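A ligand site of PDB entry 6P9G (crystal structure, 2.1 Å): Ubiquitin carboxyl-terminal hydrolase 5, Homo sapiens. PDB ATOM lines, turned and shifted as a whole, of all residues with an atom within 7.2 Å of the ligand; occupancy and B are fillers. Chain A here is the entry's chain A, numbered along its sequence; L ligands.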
ATOM      1  N   ASN A  38     -30.706 -13.287  16.265  1.00  0.00           N
ATOM      2  CA  ASN A  38     -30.284 -11.864  16.390  1.00  0.00           C
ATOM      3  C   ASN A  38     -29.812 -11.614  17.834  1.00  0.00           C
ATOM      4  O   ASN A  38     -30.206 -10.601  18.406  1.00  0.00           O
ATOM      5  CB  ASN A  38     -31.406 -10.853  16.098  1.00  0.00           C
ATOM      6  CG  ASN A  38     -32.028 -10.925  14.725  1.00  0.00           C
ATOM      7  OD1 ASN A  38     -31.572 -11.649  13.831  1.00  0.00           O
ATOM      8  ND2 ASN A  38     -33.075 -10.146  14.534  1.00  0.00           N
ATOM      9  N   TRP A  40     -26.655 -10.525  20.162  1.00  0.00           N
ATOM     10  CA  TRP A  40     -25.432  -9.699  20.107  1.00  0.00           C
ATOM     11  C   TRP A  40     -24.657  -9.706  21.449  1.00  0.00           C
ATOM     12  O   TRP A  40     -25.224  -9.370  22.529  1.00  0.00           O
ATOM     13  CB  TRP A  40     -25.837  -8.270  19.727  1.00  0.00           C
ATOM     14  CG  TRP A  40     -26.494  -8.226  18.389  1.00  0.00           C
ATOM     15  CD1 TRP A  40     -27.790  -8.530  18.116  1.00  0.00           C
ATOM     16  CD2 TRP A  40     -25.862  -7.989  17.127  1.00  0.00           C
ATOM     17  NE1 TRP A  40     -28.017  -8.440  16.769  1.00  0.00           N
ATOM     18  CE2 TRP A  40     -26.865  -8.081  16.136  1.00  0.00           C
ATOM     19  CE3 TRP A  40     -24.557  -7.652  16.727  1.00  0.00           C
ATOM     20  CZ2 TRP A  40     -26.610  -7.882  14.782  1.00  0.00           C
ATOM     21  CZ3 TRP A  40     -24.325  -7.405  15.397  1.00  0.00           C
ATOM     22  CH2 TRP A  40     -25.319  -7.519  14.441  1.00  0.00           C
ATOM     23  N   LEU A  49     -27.537 -10.294  24.367  1.00  0.00           N
ATOM     24  CA  LEU A  49     -28.862  -9.618  24.331  1.00  0.00           C
ATOM     25  C   LEU A  49     -29.354  -9.549  22.888  1.00  0.00           C
ATOM     26  O   LEU A  49     -28.513  -9.496  21.963  1.00  0.00           O
ATOM     27  CB  LEU A  49     -28.713  -8.203  24.913  1.00  0.00           C
ATOM     28  CG  LEU A  49     -28.314  -8.129  26.394  1.00  0.00           C
ATOM     29  CD1 LEU A  49     -28.075  -6.660  26.805  1.00  0.00           C
ATOM     30  CD2 LEU A  49     -29.363  -8.745  27.288  1.00  0.00           C
ATOM     31  N   CYS A  50     -30.682  -9.518  22.689  1.00  0.00           N
ATOM     32  CA  CYS A  50     -31.335  -9.634  21.364  1.00  0.00           C
ATOM     33  C   CYS A  50     -31.296  -8.321  20.578  1.00  0.00           C
ATOM     34  O   CYS A  50     -31.206  -7.201  21.184  1.00  0.00           O
ATOM     35  CB  CYS A  50     -32.755 -10.187  21.539  1.00  0.00           C
ATOM     36  SG  CYS A  50     -33.830  -9.135  22.551  1.00  0.00           S
ATOM     37  N   GLY A  51     -31.325  -8.450  19.242  1.00  0.00           N
ATOM     38  CA  GLY A  51     -31.330  -7.351  18.257  1.00  0.00           C
ATOM     39  C   GLY A  51     -32.647  -6.584  18.225  1.00  0.00           C
ATOM     40  O   GLY A  51     -33.589  -6.946  18.970  1.00  0.00           O
ATOM     41  N   ARG A  52     -32.699  -5.517  17.425  1.00  0.00           N
ATOM     42  CA  ARG A  52     -33.850  -4.579  17.372  1.00  0.00           C
ATOM     43  C   ARG A  52     -35.097  -5.342  16.907  1.00  0.00           C
ATOM     44  O   ARG A  52     -34.957  -6.353  16.183  1.00  0.00           O
ATOM     45  CB  ARG A  52     -33.588  -3.416  16.422  1.00  0.00           C
ATOM     46  CG  ARG A  52     -32.792  -2.264  17.015  1.00  0.00           C
ATOM     47  CD  ARG A  52     -32.497  -1.271  15.900  1.00  0.00           C
ATOM     48  NE  ARG A  52     -31.672  -0.128  16.300  1.00  0.00           N
ATOM     49  CZ  ARG A  52     -32.124   1.012  16.858  1.00  0.00           C
ATOM     50  NH1 ARG A  52     -31.286   1.991  17.144  1.00  0.00           N
ATOM     51  NH2 ARG A  52     -33.405   1.163  17.165  1.00  0.00           N
ATOM     52  N   ARG A  53     -36.282  -4.858  17.282  1.00  0.00           N
ATOM     53  CA  ARG A  53     -37.573  -5.402  16.786  1.00  0.00           C
ATOM     54  C   ARG A  53     -37.777  -4.915  15.350  1.00  0.00           C
ATOM     55  O   ARG A  53     -37.439  -3.779  15.068  1.00  0.00           O
ATOM     56  CB  ARG A  53     -38.708  -5.013  17.743  1.00  0.00           C
ATOM     57  CG  ARG A  53     -40.085  -5.484  17.310  1.00  0.00           C
ATOM     58  CD  ARG A  53     -41.099  -5.173  18.371  1.00  0.00           C
ATOM     59  NE  ARG A  53     -40.813  -6.013  19.519  1.00  0.00           N
ATOM     60  CZ  ARG A  53     -40.901  -5.636  20.787  1.00  0.00           C
ATOM     61  NH1 ARG A  53     -41.310  -4.421  21.092  1.00  0.00           N
ATOM     62  NH2 ARG A  53     -40.537  -6.473  21.747  1.00  0.00           N
ATOM     63  N   TYR A  54     -38.255  -5.784  14.466  1.00  0.00           N
ATOM     64  CA  TYR A  54     -38.599  -5.427  13.065  1.00  0.00           C
ATOM     65  C   TYR A  54     -39.915  -4.652  13.062  1.00  0.00           C
ATOM     66  O   TYR A  54     -40.652  -4.733  14.066  1.00  0.00           O
ATOM     67  CB  TYR A  54     -38.641  -6.683  12.203  1.00  0.00           C
ATOM     68  CG  TYR A  54     -37.322  -7.388  12.011  1.00  0.00           C
ATOM     69  CD1 TYR A  54     -36.125  -6.685  11.987  1.00  0.00           C
ATOM     70  CD2 TYR A  54     -37.268  -8.760  11.813  1.00  0.00           C
ATOM     71  CE1 TYR A  54     -34.917  -7.336  11.781  1.00  0.00           C
ATOM     72  CE2 TYR A  54     -36.066  -9.422  11.614  1.00  0.00           C
ATOM     73  CZ  TYR A  54     -34.890  -8.700  11.612  1.00  0.00           C
ATOM     74  OH  TYR A  54     -33.706  -9.332  11.373  1.00  0.00           O
ATOM     75  N   ASN A  62     -35.277  -5.682  21.334  1.00  0.00           N
ATOM     76  CA  ASN A  62     -34.538  -4.405  21.531  1.00  0.00           C
ATOM     77  C   ASN A  62     -33.602  -4.467  22.744  1.00  0.00           C
ATOM     78  O   ASN A  62     -33.169  -3.389  23.185  1.00  0.00           O
ATOM     79  CB  ASN A  62     -35.538  -3.238  21.709  1.00  0.00           C
ATOM     80  CG  ASN A  62     -36.362  -3.058  20.462  1.00  0.00           C
ATOM     81  OD1 ASN A  62     -35.819  -3.114  19.360  1.00  0.00           O
ATOM     82  ND2 ASN A  62     -37.664  -2.881  20.615  1.00  0.00           N
ATOM     83  N   HIS A  63     -33.269  -5.646  23.272  1.00  0.00           N
ATOM     84  CA  HIS A  63     -32.495  -5.690  24.542  1.00  0.00           C
ATOM     85  C   HIS A  63     -31.044  -5.185  24.350  1.00  0.00           C
ATOM     86  O   HIS A  63     -30.563  -4.506  25.232  1.00  0.00           O
ATOM     87  CB  HIS A  63     -32.663  -7.047  25.246  1.00  0.00           C
ATOM     88  CG  HIS A  63     -34.040  -7.273  25.767  1.00  0.00           C
ATOM     89  ND1 HIS A  63     -34.696  -8.478  25.612  1.00  0.00           N
ATOM     90  CD2 HIS A  63     -34.901  -6.453  26.434  1.00  0.00           C
ATOM     91  CE1 HIS A  63     -35.907  -8.385  26.169  1.00  0.00           C
ATOM     92  NE2 HIS A  63     -36.040  -7.153  26.676  1.00  0.00           N
ATOM     93  N   ALA A  64     -30.386  -5.423  23.214  1.00  0.00           N
ATOM     94  CA  ALA A  64     -28.994  -5.010  22.999  1.00  0.00           C
ATOM     95  C   ALA A  64     -28.929  -3.494  22.830  1.00  0.00           C
ATOM     96  O   ALA A  64     -28.047  -2.837  23.397  1.00  0.00           O
ATOM     97  CB  ALA A  64     -28.437  -5.723  21.789  1.00  0.00           C
ATOM     98  N   VAL A  65     -29.858  -2.931  22.057  1.00  0.00           N
ATOM     99  CA  VAL A  65     -29.865  -1.465  21.791  1.00  0.00           C
ATOM    100  C   VAL A  65     -30.285  -0.747  23.072  1.00  0.00           C
ATOM    101  O   VAL A  65     -29.623   0.239  23.401  1.00  0.00           O
ATOM    102  CB  VAL A  65     -30.735  -1.078  20.590  1.00  0.00           C
ATOM    103  CG1 VAL A  65     -32.205  -1.365  20.814  1.00  0.00           C
ATOM    104  CG2 VAL A  65     -30.484   0.360  20.176  1.00  0.00           C
ATOM    105  N   GLU A  66     -31.268  -1.242  23.820  1.00  0.00           N
ATOM    106  CA  GLU A  66     -31.616  -0.643  25.143  1.00  0.00           C
ATOM    107  C   GLU A  66     -30.358  -0.610  26.021  1.00  0.00           C
ATOM    108  O   GLU A  66     -30.014   0.479  26.531  1.00  0.00           O
ATOM    109  CB  GLU A  66     -32.787  -1.365  25.804  1.00  0.00           C
ATOM    110  CG  GLU A  66     -34.101  -1.040  25.142  1.00  0.00           C
ATOM    111  CD  GLU A  66     -35.297  -1.825  25.623  1.00  0.00           C
ATOM    112  OE1 GLU A  66     -35.140  -2.642  26.572  1.00  0.00           O
ATOM    113  OE2 GLU A  66     -36.395  -1.612  25.054  1.00  0.00           O
ATOM    114  N   ALA A  76     -20.877  -4.501  19.339  1.00  0.00           N
ATOM    115  CA  ALA A  76     -21.533  -5.786  19.627  1.00  0.00           C
ATOM    116  C   ALA A  76     -21.296  -6.709  18.428  1.00  0.00           C
ATOM    117  O   ALA A  76     -21.264  -6.220  17.252  1.00  0.00           O
ATOM    118  CB  ALA A  76     -23.000  -5.587  19.944  1.00  0.00           C
ATOM    119  N   VAL A  77     -21.136  -7.986  18.719  1.00  0.00           N
ATOM    120  CA  VAL A  77     -20.819  -8.971  17.670  1.00  0.00           C
ATOM    121  C   VAL A  77     -21.970  -9.963  17.694  1.00  0.00           C
ATOM    122  O   VAL A  77     -22.439 -10.304  18.810  1.00  0.00           O
ATOM    123  CB  VAL A  77     -19.445  -9.652  17.860  1.00  0.00           C
ATOM    124  CG1 VAL A  77     -19.376 -10.450  19.139  1.00  0.00           C
ATOM    125  CG2 VAL A  77     -19.108 -10.559  16.686  1.00  0.00           C
ATOM    126  N   LYS A  78     -22.432 -10.354  16.491  1.00  0.00           N
ATOM    127  CA  LYS A  78     -23.628 -11.189  16.325  1.00  0.00           C
ATOM    128  C   LYS A  78     -23.168 -12.631  16.440  1.00  0.00           C
ATOM    129  O   LYS A  78     -22.386 -13.096  15.573  1.00  0.00           O
ATOM    130  CB  LYS A  78     -24.324 -10.966  14.982  1.00  0.00           C
ATOM    131  CG  LYS A  78     -25.568 -11.833  14.810  1.00  0.00           C
ATOM    132  CD  LYS A  78     -26.359 -11.481  13.597  1.00  0.00           C
ATOM    133  CE  LYS A  78     -27.520 -12.434  13.425  1.00  0.00           C
ATOM    134  NZ  LYS A  78     -28.382 -12.020  12.288  1.00  0.00           N
ATOM    135  N   VAL A  89     -19.890  -7.379  13.134  1.00  0.00           N
ATOM    136  CA  VAL A  89     -19.717  -6.480  14.287  1.00  0.00           C
ATOM    137  C   VAL A  89     -20.452  -5.185  13.971  1.00  0.00           C
ATOM    138  O   VAL A  89     -20.159  -4.606  12.908  1.00  0.00           O
ATOM    139  CB  VAL A  89     -18.239  -6.218  14.599  1.00  0.00           C
ATOM    140  CG1 VAL A  89     -18.108  -5.376  15.843  1.00  0.00           C
ATOM    141  CG2 VAL A  89     -17.460  -7.512  14.736  1.00  0.00           C
ATOM    142  N   TYR A  90     -21.364  -4.779  14.862  1.00  0.00           N
ATOM    143  CA  TYR A  90     -22.106  -3.513  14.730  1.00  0.00           C
ATOM    144  C   TYR A  90     -21.575  -2.506  15.731  1.00  0.00           C
ATOM    145  O   TYR A  90     -21.297  -2.865  16.893  1.00  0.00           O
ATOM    146  CB  TYR A  90     -23.595  -3.749  14.900  1.00  0.00           C
ATOM    147  CG  TYR A  90     -24.436  -2.525  14.685  1.00  0.00           C
ATOM    148  CD1 TYR A  90     -24.622  -2.004  13.420  1.00  0.00           C
ATOM    149  CD2 TYR A  90     -24.975  -1.835  15.758  1.00  0.00           C
ATOM    150  CE1 TYR A  90     -25.372  -0.865  13.211  1.00  0.00           C
ATOM    151  CE2 TYR A  90     -25.726  -0.686  15.564  1.00  0.00           C
ATOM    152  CZ  TYR A  90     -25.945  -0.208  14.291  1.00  0.00           C
ATOM    153  OH  TYR A  90     -26.660   0.933  14.088  1.00  0.00           O
ATOM    154  N   SER A  91     -21.505  -1.248  15.310  1.00  0.00           N
ATOM    155  CA  SER A  91     -21.129  -0.114  16.181  1.00  0.00           C
ATOM    156  C   SER A  91     -22.330   0.842  16.315  1.00  0.00           C
ATOM    157  O   SER A  91     -22.793   1.414  15.304  1.00  0.00           O
ATOM    158  CB  SER A  91     -19.914   0.583  15.681  1.00  0.00           C
ATOM    159  OG  SER A  91     -19.760   1.834  16.333  1.00  0.00           O
ATOM    160  N   TYR A  92     -22.837   0.965  17.539  1.00  0.00           N
ATOM    161  CA  TYR A  92     -24.056   1.731  17.843  1.00  0.00           C
ATOM    162  C   TYR A  92     -23.753   3.209  17.712  1.00  0.00           C
ATOM    163  O   TYR A  92     -24.642   3.900  17.262  1.00  0.00           O
ATOM    164  CB  TYR A  92     -24.545   1.465  19.260  1.00  0.00           C
ATOM    165  CG  TYR A  92     -25.283   0.180  19.431  1.00  0.00           C
ATOM    166  CD1 TYR A  92     -26.610   0.041  19.012  1.00  0.00           C
ATOM    167  CD2 TYR A  92     -24.678  -0.896  20.031  1.00  0.00           C
ATOM    168  CE1 TYR A  92     -27.289  -1.150  19.192  1.00  0.00           C
ATOM    169  CE2 TYR A  92     -25.364  -2.088  20.218  1.00  0.00           C
ATOM    170  CZ  TYR A  92     -26.669  -2.216  19.806  1.00  0.00           C
ATOM    171  OH  TYR A  92     -27.319  -3.407  20.013  1.00  0.00           O
ATOM    172  N   ASP A  95     -23.123   3.803  13.987  1.00  0.00           N
ATOM    173  CA  ASP A  95     -24.309   3.349  13.215  1.00  0.00           C
ATOM    174  C   ASP A  95     -23.853   2.715  11.907  1.00  0.00           C
ATOM    175  O   ASP A  95     -24.269   3.182  10.846  1.00  0.00           O
ATOM    176  CB  ASP A  95     -25.350   4.453  12.952  1.00  0.00           C
ATOM    177  CG  ASP A  95     -26.621   3.939  12.273  1.00  0.00           C
ATOM    178  OD1 ASP A  95     -26.870   2.671  12.269  1.00  0.00           O
ATOM    179  OD2 ASP A  95     -27.346   4.785  11.717  1.00  0.00           O
ATOM    180  N   ASP A  96     -23.103   1.632  11.997  1.00  0.00           N
ATOM    181  CA  ASP A  96     -22.639   0.852  10.831  1.00  0.00           C
ATOM    182  C   ASP A  96     -22.163  -0.525  11.281  1.00  0.00           C
ATOM    183  O   ASP A  96     -21.811  -0.671  12.465  1.00  0.00           O
ATOM    184  CB  ASP A  96     -21.475   1.536  10.106  1.00  0.00           C
ATOM    185  CG  ASP A  96     -21.908   2.281   8.868  1.00  0.00           C
ATOM    186  OD1 ASP A  96     -22.820   1.799   8.168  1.00  0.00           O
ATOM    187  OD2 ASP A  96     -21.308   3.331   8.614  1.00  0.00           O
ATOM    188  N   MET A  97     -22.149  -1.463  10.353  1.00  0.00           N
ATOM    189  CA  MET A  97     -21.360  -2.706  10.464  1.00  0.00           C
ATOM    190  C   MET A  97     -19.906  -2.241  10.283  1.00  0.00           C
ATOM    191  O   MET A  97     -19.659  -1.383   9.412  1.00  0.00           O
ATOM    192  CB  MET A  97     -21.762  -3.744   9.428  1.00  0.00           C
ATOM    193  CG  MET A  97     -23.240  -4.143   9.456  1.00  0.00           C
ATOM    194  SD  MET A  97     -23.788  -4.861  11.033  1.00  0.00           S
ATOM    195  CE  MET A  97     -22.539  -6.096  11.338  1.00  0.00           C
HETATM  196  C1  LIG L   1     -26.971  -4.776  16.948  1.00  0.00           C
HETATM  197  C2  LIG L   1     -28.112  -3.796  16.634  1.00  0.00           C
HETATM  198  C3  LIG L   1     -29.466  -4.253  17.208  1.00  0.00           C
HETATM  199  O1  LIG L   1     -29.653  -4.012  18.452  1.00  0.00           O
HETATM  200  O2  LIG L   1     -30.259  -4.784  16.409  1.00  0.00           O
HETATM  201  N1  LIG L   1     -28.164  -3.500  15.197  1.00  0.00           N
HETATM  202  C4  LIG L   1     -27.675  -4.412  14.301  1.00  0.00           C
HETATM  203  N2  LIG L   1     -27.633  -4.269  13.030  1.00  0.00           N
HETATM  204  C5  LIG L   1     -28.080  -3.058  12.522  1.00  0.00           C
HETATM  205  C6  LIG L   1     -28.011  -2.858  11.132  1.00  0.00           C
HETATM  206  C7  LIG L   1     -28.401  -1.662  10.593  1.00  0.00           C
HETATM  207  C8  LIG L   1     -28.900  -0.637  11.410  1.00  0.00           C
HETATM  208  C9  LIG L   1     -29.014  -0.818  12.774  1.00  0.00           C
HETATM  209  C10 LIG L   1     -28.572  -2.033  13.346  1.00  0.00           C
HETATM  210  C11 LIG L   1     -28.624  -2.254  14.790  1.00  0.00           C
HETATM  211  O3  LIG L   1     -29.059  -1.447  15.617  1.00  0.00           O
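The backbone NH of Arg 52 is in hydrogen-bond range of an oxygen (O2) of the ligand, 2.7 Å away.
An oxygen (O1) of the ligand is in hydrogen-bond range of the side-chain hydroxyl of Tyr 92 (2.9 Å).
The guanidinium group of Arg 52 is in hydrogen-bond range of an oxygen (O3) of the ligand (3.0 Å).
O of Gly 51 is in hydrogen-bond range of N of Asn 62, at 3.2 Å.
The side-chain hydroxyl of Tyr 90 lies within hydrogen-bond range of the side-chain carboxylate of Asp 95.
The backbone carbonyl oxygen (O) of Asn 38 lies close to the indole nitrogen (NE1) of Trp 40.
The backbone NH of Ala 64 sits at hydrogen-bond distance from the backbone carbonyl oxygen of Cys 50, at 2.8 Å.
The backbone carbonyl oxygen (O) of Ala 76 is in hydrogen-bond range of the backbone NH (N) of Tyr 90, at 2.8 Å.
The side-chain hydroxyl of Tyr 92 is in hydrogen-bond range of the backbone NH of Val 65 (3.3 Å).
The backbone NH (N) of Gly 51 lies within hydrogen-bond range of the backbone carbonyl oxygen (O) of Asn 38.
O of Leu 49 sits at hydrogen-bond distance from N of Trp 40, at 2.8 Å.
Trp 40 touches the ligand (CD2 to C1, 3.4 Å).
Gly 51 touches the ligand.
CB of Ala 64 touches O1 of the ligand, 3.9 Å away.
N of Val 65 touches O1 of the ligand (3.8 Å).
Tyr 90 touches the ligand (OH to C9, 3.2 Å).
Asp 95 touches the ligand.
Hydrophobic or aromatic side chains within 4 Å of the ligand: Trp 40, Ala 64, Val 65, Tyr 90 and Tyr 92.
Eight residues have an atom within 4 Å of the ligand: Trp 40, Gly 51, Arg 52, Ala 64, Val 65, Tyr 90, Tyr 92 and Asp 95.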
